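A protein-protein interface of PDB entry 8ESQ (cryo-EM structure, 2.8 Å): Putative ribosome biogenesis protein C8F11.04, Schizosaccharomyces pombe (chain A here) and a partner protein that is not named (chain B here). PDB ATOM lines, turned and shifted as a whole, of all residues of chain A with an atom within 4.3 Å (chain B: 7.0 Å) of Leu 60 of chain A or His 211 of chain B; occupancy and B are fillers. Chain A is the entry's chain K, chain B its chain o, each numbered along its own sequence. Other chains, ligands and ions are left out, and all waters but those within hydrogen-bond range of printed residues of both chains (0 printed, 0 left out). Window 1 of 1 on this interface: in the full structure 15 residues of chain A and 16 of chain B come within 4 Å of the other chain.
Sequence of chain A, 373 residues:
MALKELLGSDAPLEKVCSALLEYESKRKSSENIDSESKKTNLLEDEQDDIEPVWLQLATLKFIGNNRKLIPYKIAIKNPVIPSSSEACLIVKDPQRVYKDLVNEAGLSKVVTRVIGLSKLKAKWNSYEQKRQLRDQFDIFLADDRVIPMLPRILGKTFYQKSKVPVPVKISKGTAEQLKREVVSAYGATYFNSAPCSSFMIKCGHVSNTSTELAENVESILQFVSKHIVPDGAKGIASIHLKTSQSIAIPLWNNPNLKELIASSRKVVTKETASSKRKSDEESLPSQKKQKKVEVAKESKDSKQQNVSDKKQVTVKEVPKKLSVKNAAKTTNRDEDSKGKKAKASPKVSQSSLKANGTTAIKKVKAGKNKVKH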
ATOM      1  N   THR A  59      14.648  -6.424  11.521  1.00  0.00           N
ATOM      2  CA  THR A  59      13.479  -6.449  10.655  1.00  0.00           C
ATOM      3  C   THR A  59      12.433  -5.464  11.162  1.00  0.00           C
ATOM      4  O   THR A  59      12.530  -4.924  12.267  1.00  0.00           O
ATOM      5  CB  THR A  59      12.886  -7.859  10.578  1.00  0.00           C
ATOM      6  OG1 THR A  59      12.334  -8.215  11.852  1.00  0.00           O
ATOM      7  CG2 THR A  59      13.956  -8.866  10.194  1.00  0.00           C
ATOM      8  N   LEU A  60      11.423  -5.233  10.329  1.00  0.00           N
ATOM      9  CA  LEU A  60      10.340  -4.319  10.663  1.00  0.00           C
ATOM     10  C   LEU A  60       9.199  -5.004  11.401  1.00  0.00           C
ATOM     11  O   LEU A  60       8.248  -4.328  11.806  1.00  0.00           O
ATOM     12  CB  LEU A  60       9.809  -3.651   9.393  1.00  0.00           C
ATOM     13  CG  LEU A  60      10.818  -2.754   8.672  1.00  0.00           C
ATOM     14  CD1 LEU A  60      10.338  -2.413   7.268  1.00  0.00           C
ATOM     15  CD2 LEU A  60      11.099  -1.496   9.475  1.00  0.00           C
ATOM     16  N   LYS A  61       9.271  -6.320  11.589  1.00  0.00           N
ATOM     17  CA  LYS A  61       8.262  -7.054  12.336  1.00  0.00           C
ATOM     18  C   LYS A  61       8.895  -8.324  12.880  1.00  0.00           C
ATOM     19  O   LYS A  61       9.950  -8.762  12.413  1.00  0.00           O
ATOM     20  CB  LYS A  61       7.039  -7.373  11.473  1.00  0.00           C
ATOM     21  CG  LYS A  61       7.329  -8.285  10.303  1.00  0.00           C
ATOM     22  CD  LYS A  61       6.160  -8.308   9.339  1.00  0.00           C
ATOM     23  CE  LYS A  61       6.406  -9.288   8.215  1.00  0.00           C
ATOM     24  NZ  LYS A  61       7.629  -8.933   7.447  1.00  0.00           N
ATOM     25  N   PHE A  62       8.237  -8.911  13.878  1.00  0.00           N
ATOM     26  CA  PHE A  62       8.751 -10.114  14.525  1.00  0.00           C
ATOM     27  C   PHE A  62       8.667 -11.279  13.549  1.00  0.00           C
ATOM     28  O   PHE A  62       7.571 -11.711  13.175  1.00  0.00           O
ATOM     29  CB  PHE A  62       7.971 -10.409  15.804  1.00  0.00           C
ATOM     30  CG  PHE A  62       8.405  -9.589  16.992  1.00  0.00           C
ATOM     31  CD1 PHE A  62       9.047  -8.373  16.826  1.00  0.00           C
ATOM     32  CD2 PHE A  62       8.180 -10.048  18.278  1.00  0.00           C
ATOM     33  CE1 PHE A  62       9.441  -7.626  17.922  1.00  0.00           C
ATOM     34  CE2 PHE A  62       8.574  -9.307  19.375  1.00  0.00           C
ATOM     35  CZ  PHE A  62       9.205  -8.095  19.197  1.00  0.00           C
ATOM     36  N   SER A 197      12.475  -8.972  16.632  1.00  0.00           N
ATOM     37  CA  SER A 197      12.691  -8.175  15.433  1.00  0.00           C
ATOM     38  C   SER A 197      14.135  -8.198  14.963  1.00  0.00           C
ATOM     39  O   SER A 197      14.387  -8.035  13.763  1.00  0.00           O
ATOM     40  CB  SER A 197      12.270  -6.726  15.683  1.00  0.00           C
ATOM     41  OG  SER A 197      12.987  -6.170  16.770  1.00  0.00           O
ATOM     42  N   LYS A 234      12.427  -5.737   1.765  1.00  0.00           N
ATOM     43  CA  LYS A 234      11.425  -4.770   2.205  1.00  0.00           C
ATOM     44  C   LYS A 234      11.103  -4.939   3.686  1.00  0.00           C
ATOM     45  O   LYS A 234      10.832  -3.955   4.383  1.00  0.00           O
ATOM     46  CB  LYS A 234      10.147  -4.856   1.354  1.00  0.00           C
ATOM     47  CG  LYS A 234      10.268  -4.530  -0.159  1.00  0.00           C
ATOM     48  CD  LYS A 234      11.172  -5.400  -1.039  1.00  0.00           C
ATOM     49  CE  LYS A 234      11.067  -6.878  -0.741  1.00  0.00           C
ATOM     50  NZ  LYS A 234      12.163  -7.659  -1.381  1.00  0.00           N
ATOM     51  N   GLY A 235      11.124  -6.175   4.188  1.00  0.00           N
ATOM     52  CA  GLY A 235      10.991  -6.382   5.621  1.00  0.00           C
ATOM     53  C   GLY A 235      12.236  -6.031   6.410  1.00  0.00           C
ATOM     54  O   GLY A 235      12.137  -5.720   7.601  1.00  0.00           O
ATOM     55  N   ALA A 237      15.179  -3.989   8.006  1.00  0.00           N
ATOM     56  CA  ALA A 237      15.383  -2.622   8.469  1.00  0.00           C
ATOM     57  C   ALA A 237      16.841  -2.184   8.379  1.00  0.00           C
ATOM     58  O   ALA A 237      17.145  -1.179   7.733  1.00  0.00           O
ATOM     59  CB  ALA A 237      14.880  -2.474   9.910  1.00  0.00           C
ATOM     60  N   LEU A 260       8.188   2.608   4.271  1.00  0.00           N
ATOM     61  CA  LEU A 260       7.807   1.241   4.613  1.00  0.00           C
ATOM     62  C   LEU A 260       7.213   1.160   6.014  1.00  0.00           C
ATOM     63  O   LEU A 260       6.224   0.452   6.235  1.00  0.00           O
ATOM     64  CB  LEU A 260       9.010   0.307   4.479  1.00  0.00           C
ATOM     65  CG  LEU A 260       9.567   0.136   3.063  1.00  0.00           C
ATOM     66  CD1 LEU A 260      10.560  -1.013   3.003  1.00  0.00           C
ATOM     67  CD2 LEU A 260       8.439  -0.075   2.063  1.00  0.00           C
ATOM     68  N   ILE A 261       7.803   1.874   6.978  1.00  0.00           N
ATOM     69  CA  ILE A 261       7.268   1.847   8.338  1.00  0.00           C
ATOM     70  C   ILE A 261       5.892   2.498   8.384  1.00  0.00           C
ATOM     71  O   ILE A 261       5.001   2.048   9.113  1.00  0.00           O
ATOM     72  CB  ILE A 261       8.249   2.507   9.329  1.00  0.00           C
ATOM     73  CG1 ILE A 261       8.410   4.003   9.040  1.00  0.00           C
ATOM     74  CG2 ILE A 261       9.590   1.792   9.318  1.00  0.00           C
ATOM     75  CD1 ILE A 261       9.252   4.736  10.055  1.00  0.00           C
ATOM     76  N   ARG A 265       2.833   0.160   9.460  1.00  0.00           N
ATOM     77  CA  ARG A 265       2.232   0.566  10.732  1.00  0.00           C
ATOM     78  C   ARG A 265       1.043   1.500  10.499  1.00  0.00           C
ATOM     79  O   ARG A 265       1.029   2.659  10.910  1.00  0.00           O
ATOM     80  CB  ARG A 265       3.287   1.214  11.622  1.00  0.00           C
ATOM     81  CG  ARG A 265       4.390   0.274  12.080  1.00  0.00           C
ATOM     82  CD  ARG A 265       4.015  -0.418  13.382  1.00  0.00           C
ATOM     83  NE  ARG A 265       3.868   0.543  14.469  1.00  0.00           N
ATOM     84  CZ  ARG A 265       3.732   0.221  15.748  1.00  0.00           C
ATOM     85  NH1 ARG A 265       3.706  -1.039  16.144  1.00  0.00           N
ATOM     86  NH2 ARG A 265       3.619   1.188  16.653  1.00  0.00           N
ATOM     87  N   THR B 205       4.883 -11.782  23.437  1.00  0.00           N
ATOM     88  CA  THR B 205       3.644 -11.462  22.734  1.00  0.00           C
ATOM     89  C   THR B 205       3.327  -9.973  22.819  1.00  0.00           C
ATOM     90  O   THR B 205       2.967  -9.354  21.810  1.00  0.00           O
ATOM     91  CB  THR B 205       2.493 -12.295  23.298  1.00  0.00           C
ATOM     92  OG1 THR B 205       2.515 -13.601  22.710  1.00  0.00           O
ATOM     93  CG2 THR B 205       1.159 -11.643  22.991  1.00  0.00           C
ATOM     94  N   ILE B 206       3.457  -9.377  24.007  1.00  0.00           N
ATOM     95  CA  ILE B 206       3.215  -7.943  24.144  1.00  0.00           C
ATOM     96  C   ILE B 206       4.190  -7.150  23.283  1.00  0.00           C
ATOM     97  O   ILE B 206       3.798  -6.206  22.587  1.00  0.00           O
ATOM     98  CB  ILE B 206       3.285  -7.516  25.623  1.00  0.00           C
ATOM     99  CG1 ILE B 206       2.023  -7.947  26.374  1.00  0.00           C
ATOM    100  CG2 ILE B 206       3.491  -6.015  25.744  1.00  0.00           C
ATOM    101  CD1 ILE B 206       2.124  -9.281  27.053  1.00  0.00           C
ATOM    102  N   ALA B 207       5.472  -7.523  23.309  1.00  0.00           N
ATOM    103  CA  ALA B 207       6.445  -6.845  22.460  1.00  0.00           C
ATOM    104  C   ALA B 207       6.127  -7.036  20.983  1.00  0.00           C
ATOM    105  O   ALA B 207       6.403  -6.146  20.172  1.00  0.00           O
ATOM    106  CB  ALA B 207       7.856  -7.341  22.769  1.00  0.00           C
ATOM    107  N   ARG B 208       5.558  -8.185  20.618  1.00  0.00           N
ATOM    108  CA  ARG B 208       5.145  -8.404  19.234  1.00  0.00           C
ATOM    109  C   ARG B 208       4.046  -7.431  18.831  1.00  0.00           C
ATOM    110  O   ARG B 208       4.118  -6.797  17.772  1.00  0.00           O
ATOM    111  CB  ARG B 208       4.666  -9.840  19.057  1.00  0.00           C
ATOM    112  CG  ARG B 208       4.204 -10.169  17.656  1.00  0.00           C
ATOM    113  CD  ARG B 208       3.388 -11.436  17.685  1.00  0.00           C
ATOM    114  NE  ARG B 208       4.102 -12.495  18.383  1.00  0.00           N
ATOM    115  CZ  ARG B 208       4.152 -13.755  17.981  1.00  0.00           C
ATOM    116  NH1 ARG B 208       3.538 -14.153  16.878  1.00  0.00           N
ATOM    117  NH2 ARG B 208       4.831 -14.639  18.706  1.00  0.00           N
ATOM    118  N   LEU B 209       3.011  -7.311  19.663  1.00  0.00           N
ATOM    119  CA  LEU B 209       1.953  -6.348  19.383  1.00  0.00           C
ATOM    120  C   LEU B 209       2.494  -4.928  19.418  1.00  0.00           C
ATOM    121  O   LEU B 209       2.101  -4.084  18.607  1.00  0.00           O
ATOM    122  CB  LEU B 209       0.813  -6.509  20.386  1.00  0.00           C
ATOM    123  CG  LEU B 209       0.269  -7.918  20.614  1.00  0.00           C
ATOM    124  CD1 LEU B 209      -0.989  -7.834  21.451  1.00  0.00           C
ATOM    125  CD2 LEU B 209      -0.005  -8.627  19.297  1.00  0.00           C
ATOM    126  N   GLN B 210       3.397  -4.648  20.358  1.00  0.00           N
ATOM    127  CA  GLN B 210       4.028  -3.336  20.413  1.00  0.00           C
ATOM    128  C   GLN B 210       4.818  -3.059  19.139  1.00  0.00           C
ATOM    129  O   GLN B 210       4.891  -1.913  18.680  1.00  0.00           O
ATOM    130  CB  GLN B 210       4.920  -3.250  21.649  1.00  0.00           C
ATOM    131  CG  GLN B 210       4.183  -2.758  22.884  1.00  0.00           C
ATOM    132  CD  GLN B 210       5.061  -1.950  23.814  1.00  0.00           C
ATOM    133  OE1 GLN B 210       4.841  -0.756  24.013  1.00  0.00           O
ATOM    134  NE2 GLN B 210       6.058  -2.601  24.399  1.00  0.00           N
ATOM    135  N   HIS B 211       5.419  -4.098  18.555  1.00  0.00           N
ATOM    136  CA  HIS B 211       6.058  -3.950  17.251  1.00  0.00           C
ATOM    137  C   HIS B 211       5.037  -3.672  16.155  1.00  0.00           C
ATOM    138  O   HIS B 211       5.211  -2.749  15.352  1.00  0.00           O
ATOM    139  CB  HIS B 211       6.870  -5.198  16.912  1.00  0.00           C
ATOM    140  CG  HIS B 211       8.179  -4.903  16.252  1.00  0.00           C
ATOM    141  ND1 HIS B 211       9.129  -4.075  16.806  1.00  0.00           N
ATOM    142  CD2 HIS B 211       8.681  -5.308  15.062  1.00  0.00           C
ATOM    143  CE1 HIS B 211      10.168  -3.997  15.994  1.00  0.00           C
ATOM    144  NE2 HIS B 211       9.919  -4.731  14.926  1.00  0.00           N
ATOM    145  N   GLU B 212       3.959  -4.453  16.108  1.00  0.00           N
ATOM    146  CA  GLU B 212       2.969  -4.349  15.035  1.00  0.00           C
ATOM    147  C   GLU B 212       1.611  -4.021  15.647  1.00  0.00           C
ATOM    148  O   GLU B 212       0.804  -4.909  15.929  1.00  0.00           O
ATOM    149  CB  GLU B 212       2.922  -5.639  14.206  1.00  0.00           C
ATOM    150  CG  GLU B 212       4.120  -5.827  13.286  1.00  0.00           C
ATOM    151  CD  GLU B 212       4.270  -4.701  12.279  1.00  0.00           C
ATOM    152  OE1 GLU B 212       3.250  -4.275  11.697  1.00  0.00           O
ATOM    153  OE2 GLU B 212       5.412  -4.242  12.071  1.00  0.00           O
ATOM    154  N   LYS B 213       1.362  -2.733  15.839  1.00  0.00           N
ATOM    155  CA  LYS B 213       0.101  -2.193  16.315  1.00  0.00           C
ATOM    156  C   LYS B 213      -0.309  -1.030  15.423  1.00  0.00           C
ATOM    157  O   LYS B 213       0.524  -0.476  14.695  1.00  0.00           O
ATOM    158  CB  LYS B 213       0.209  -1.718  17.772  1.00  0.00           C
ATOM    159  CG  LYS B 213       1.049  -0.469  17.966  1.00  0.00           C
ATOM    160  CD  LYS B 213       1.070  -0.044  19.426  1.00  0.00           C
ATOM    161  CE  LYS B 213       1.881   1.226  19.622  1.00  0.00           C
ATOM    162  NZ  LYS B 213       1.902   1.660  21.047  1.00  0.00           N
ATOM    163  N   LEU B 215      -0.783   2.503  14.018  1.00  0.00           N
ATOM    164  CA  LEU B 215       0.106   3.641  14.190  1.00  0.00           C
ATOM    165  C   LEU B 215      -0.316   4.755  13.244  1.00  0.00           C
ATOM    166  O   LEU B 215      -0.898   4.512  12.183  1.00  0.00           O
ATOM    167  CB  LEU B 215       1.569   3.233  13.949  1.00  0.00           C
ATOM    168  CG  LEU B 215       2.691   4.273  13.987  1.00  0.00           C
ATOM    169  CD1 LEU B 215       3.925   3.725  14.665  1.00  0.00           C
ATOM    170  CD2 LEU B 215       3.031   4.679  12.570  1.00  0.00           C
ATOM    171  N   LEU B 223       8.897   7.876  15.744  1.00  0.00           N
ATOM    172  CA  LEU B 223       9.712   6.669  15.664  1.00  0.00           C
ATOM    173  C   LEU B 223      11.016   6.928  14.922  1.00  0.00           C
ATOM    174  O   LEU B 223      12.090   6.537  15.394  1.00  0.00           O
ATOM    175  CB  LEU B 223       8.926   5.544  14.984  1.00  0.00           C
ATOM    176  CG  LEU B 223       9.612   4.183  14.798  1.00  0.00           C
ATOM    177  CD1 LEU B 223       8.592   3.068  14.910  1.00  0.00           C
ATOM    178  CD2 LEU B 223      10.340   4.082  13.463  1.00  0.00           C
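O of Gln 210 of chain B sits at hydrogen-bond distance from NH1 of Arg 265 of chain A (2.9 Å).
The guanidinium group (NH1) of Arg 265 of chain A sits at hydrogen-bond distance from the backbone carbonyl oxygen (O) of His 211 of chain B, at 2.4 Å.
O of Leu 60 of chain A sits close to OE2 of Glu 212 of chain B (2.8 Å).
N of Glu 212 of chain B sits close to NH1 of Arg 265 of chain A (3.4 Å).
NH1 of Arg 265 of chain A lies close to N of Lys 213 of chain B (2.9 Å).
The backbone carbonyl oxygen of Arg 265 of chain A sits close to the backbone carbonyl oxygen of Leu 215 of chain B, 3.0 Å away.
The side-chain hydroxyl of Thr 59 of chain A is in hydrogen-bond range of the backbone carbonyl oxygen of Lys 61 of chain A (2.5 Å).
N of Thr 59 of chain A is in hydrogen-bond range of O of Ser 197 of chain A, 2.8 Å away.
The backbone NH (N) of Leu 60 of chain A sits at hydrogen-bond distance from the backbone carbonyl oxygen (O) of Gly 235 of chain A.
His 211 of chain B touches Thr 59 of chain A (NE2 to O, 3.7 Å).
Leu 60 of chain A touches His 211 of chain B.
CD2 of His 211 of chain B touches CA of Lys 61 of chain A, at 3.3 Å.
Lys 61 of chain A touches Glu 212 of chain B.
Phe 62 of chain A touches Ala 207 of chain B (CZ to O, 3.5 Å).
Phe 62 of chain A touches Arg 208 of chain B.
Phe 62 of chain A touches His 211 of chain B (CE1 to CG, 3.4 Å).
CB of Ser 197 of chain A touches NE2 of His 211 of chain B (3.2 Å).
CD2 of Leu 223 of chain B touches CD1 of Ile 261 of chain A, at 3.6 Å.
Leu 60 of chain A touches just these residues of chain B: His 211 (3.4 Å) and Glu 212 (2.8 Å).
Of the printed residues of chain B, Lys 61 of chain A touches His 211 and Glu 212.
Of the printed residues of chain B, Phe 62 of chain A touches Ala 207 (3.5 Å), Arg 208 (3.4 Å) and His 211 (3.4 Å).
Of the printed residues of chain B, Arg 265 of chain A touches Gln 210, His 211, Glu 212, Lys 213 and Leu 215.
Of the printed residues of chain A, Arg 208 of chain B touches Phe 62.
His 211 of chain B touches six residues of chain A.
Of the printed residues of chain A, Glu 212 of chain B touches Leu 60, Lys 61 and Arg 265.
The nearest printed residue of chain A that does not touch His 211 of chain B is Ala 237 of chain A (7.4 Å).
The nearest printed residue of chain B that does not touch Thr 59 of chain A is Glu 212 of chain B (7.2 Å).
Printed residues of chain A that touch a printed residue of chain B: Thr 59, Leu 60, Lys 61, Phe 62, Ser 197, Ile 261 and Arg 265.
Along chain A the printed residues that touch a printed residue of chain B span positions 59 to 265.
Printed residues of chain B that touch a printed residue of chain A: Ala 207, Arg 208, Gln 210, His 211, Glu 212, Lys 213, Leu 215 and Leu 223.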
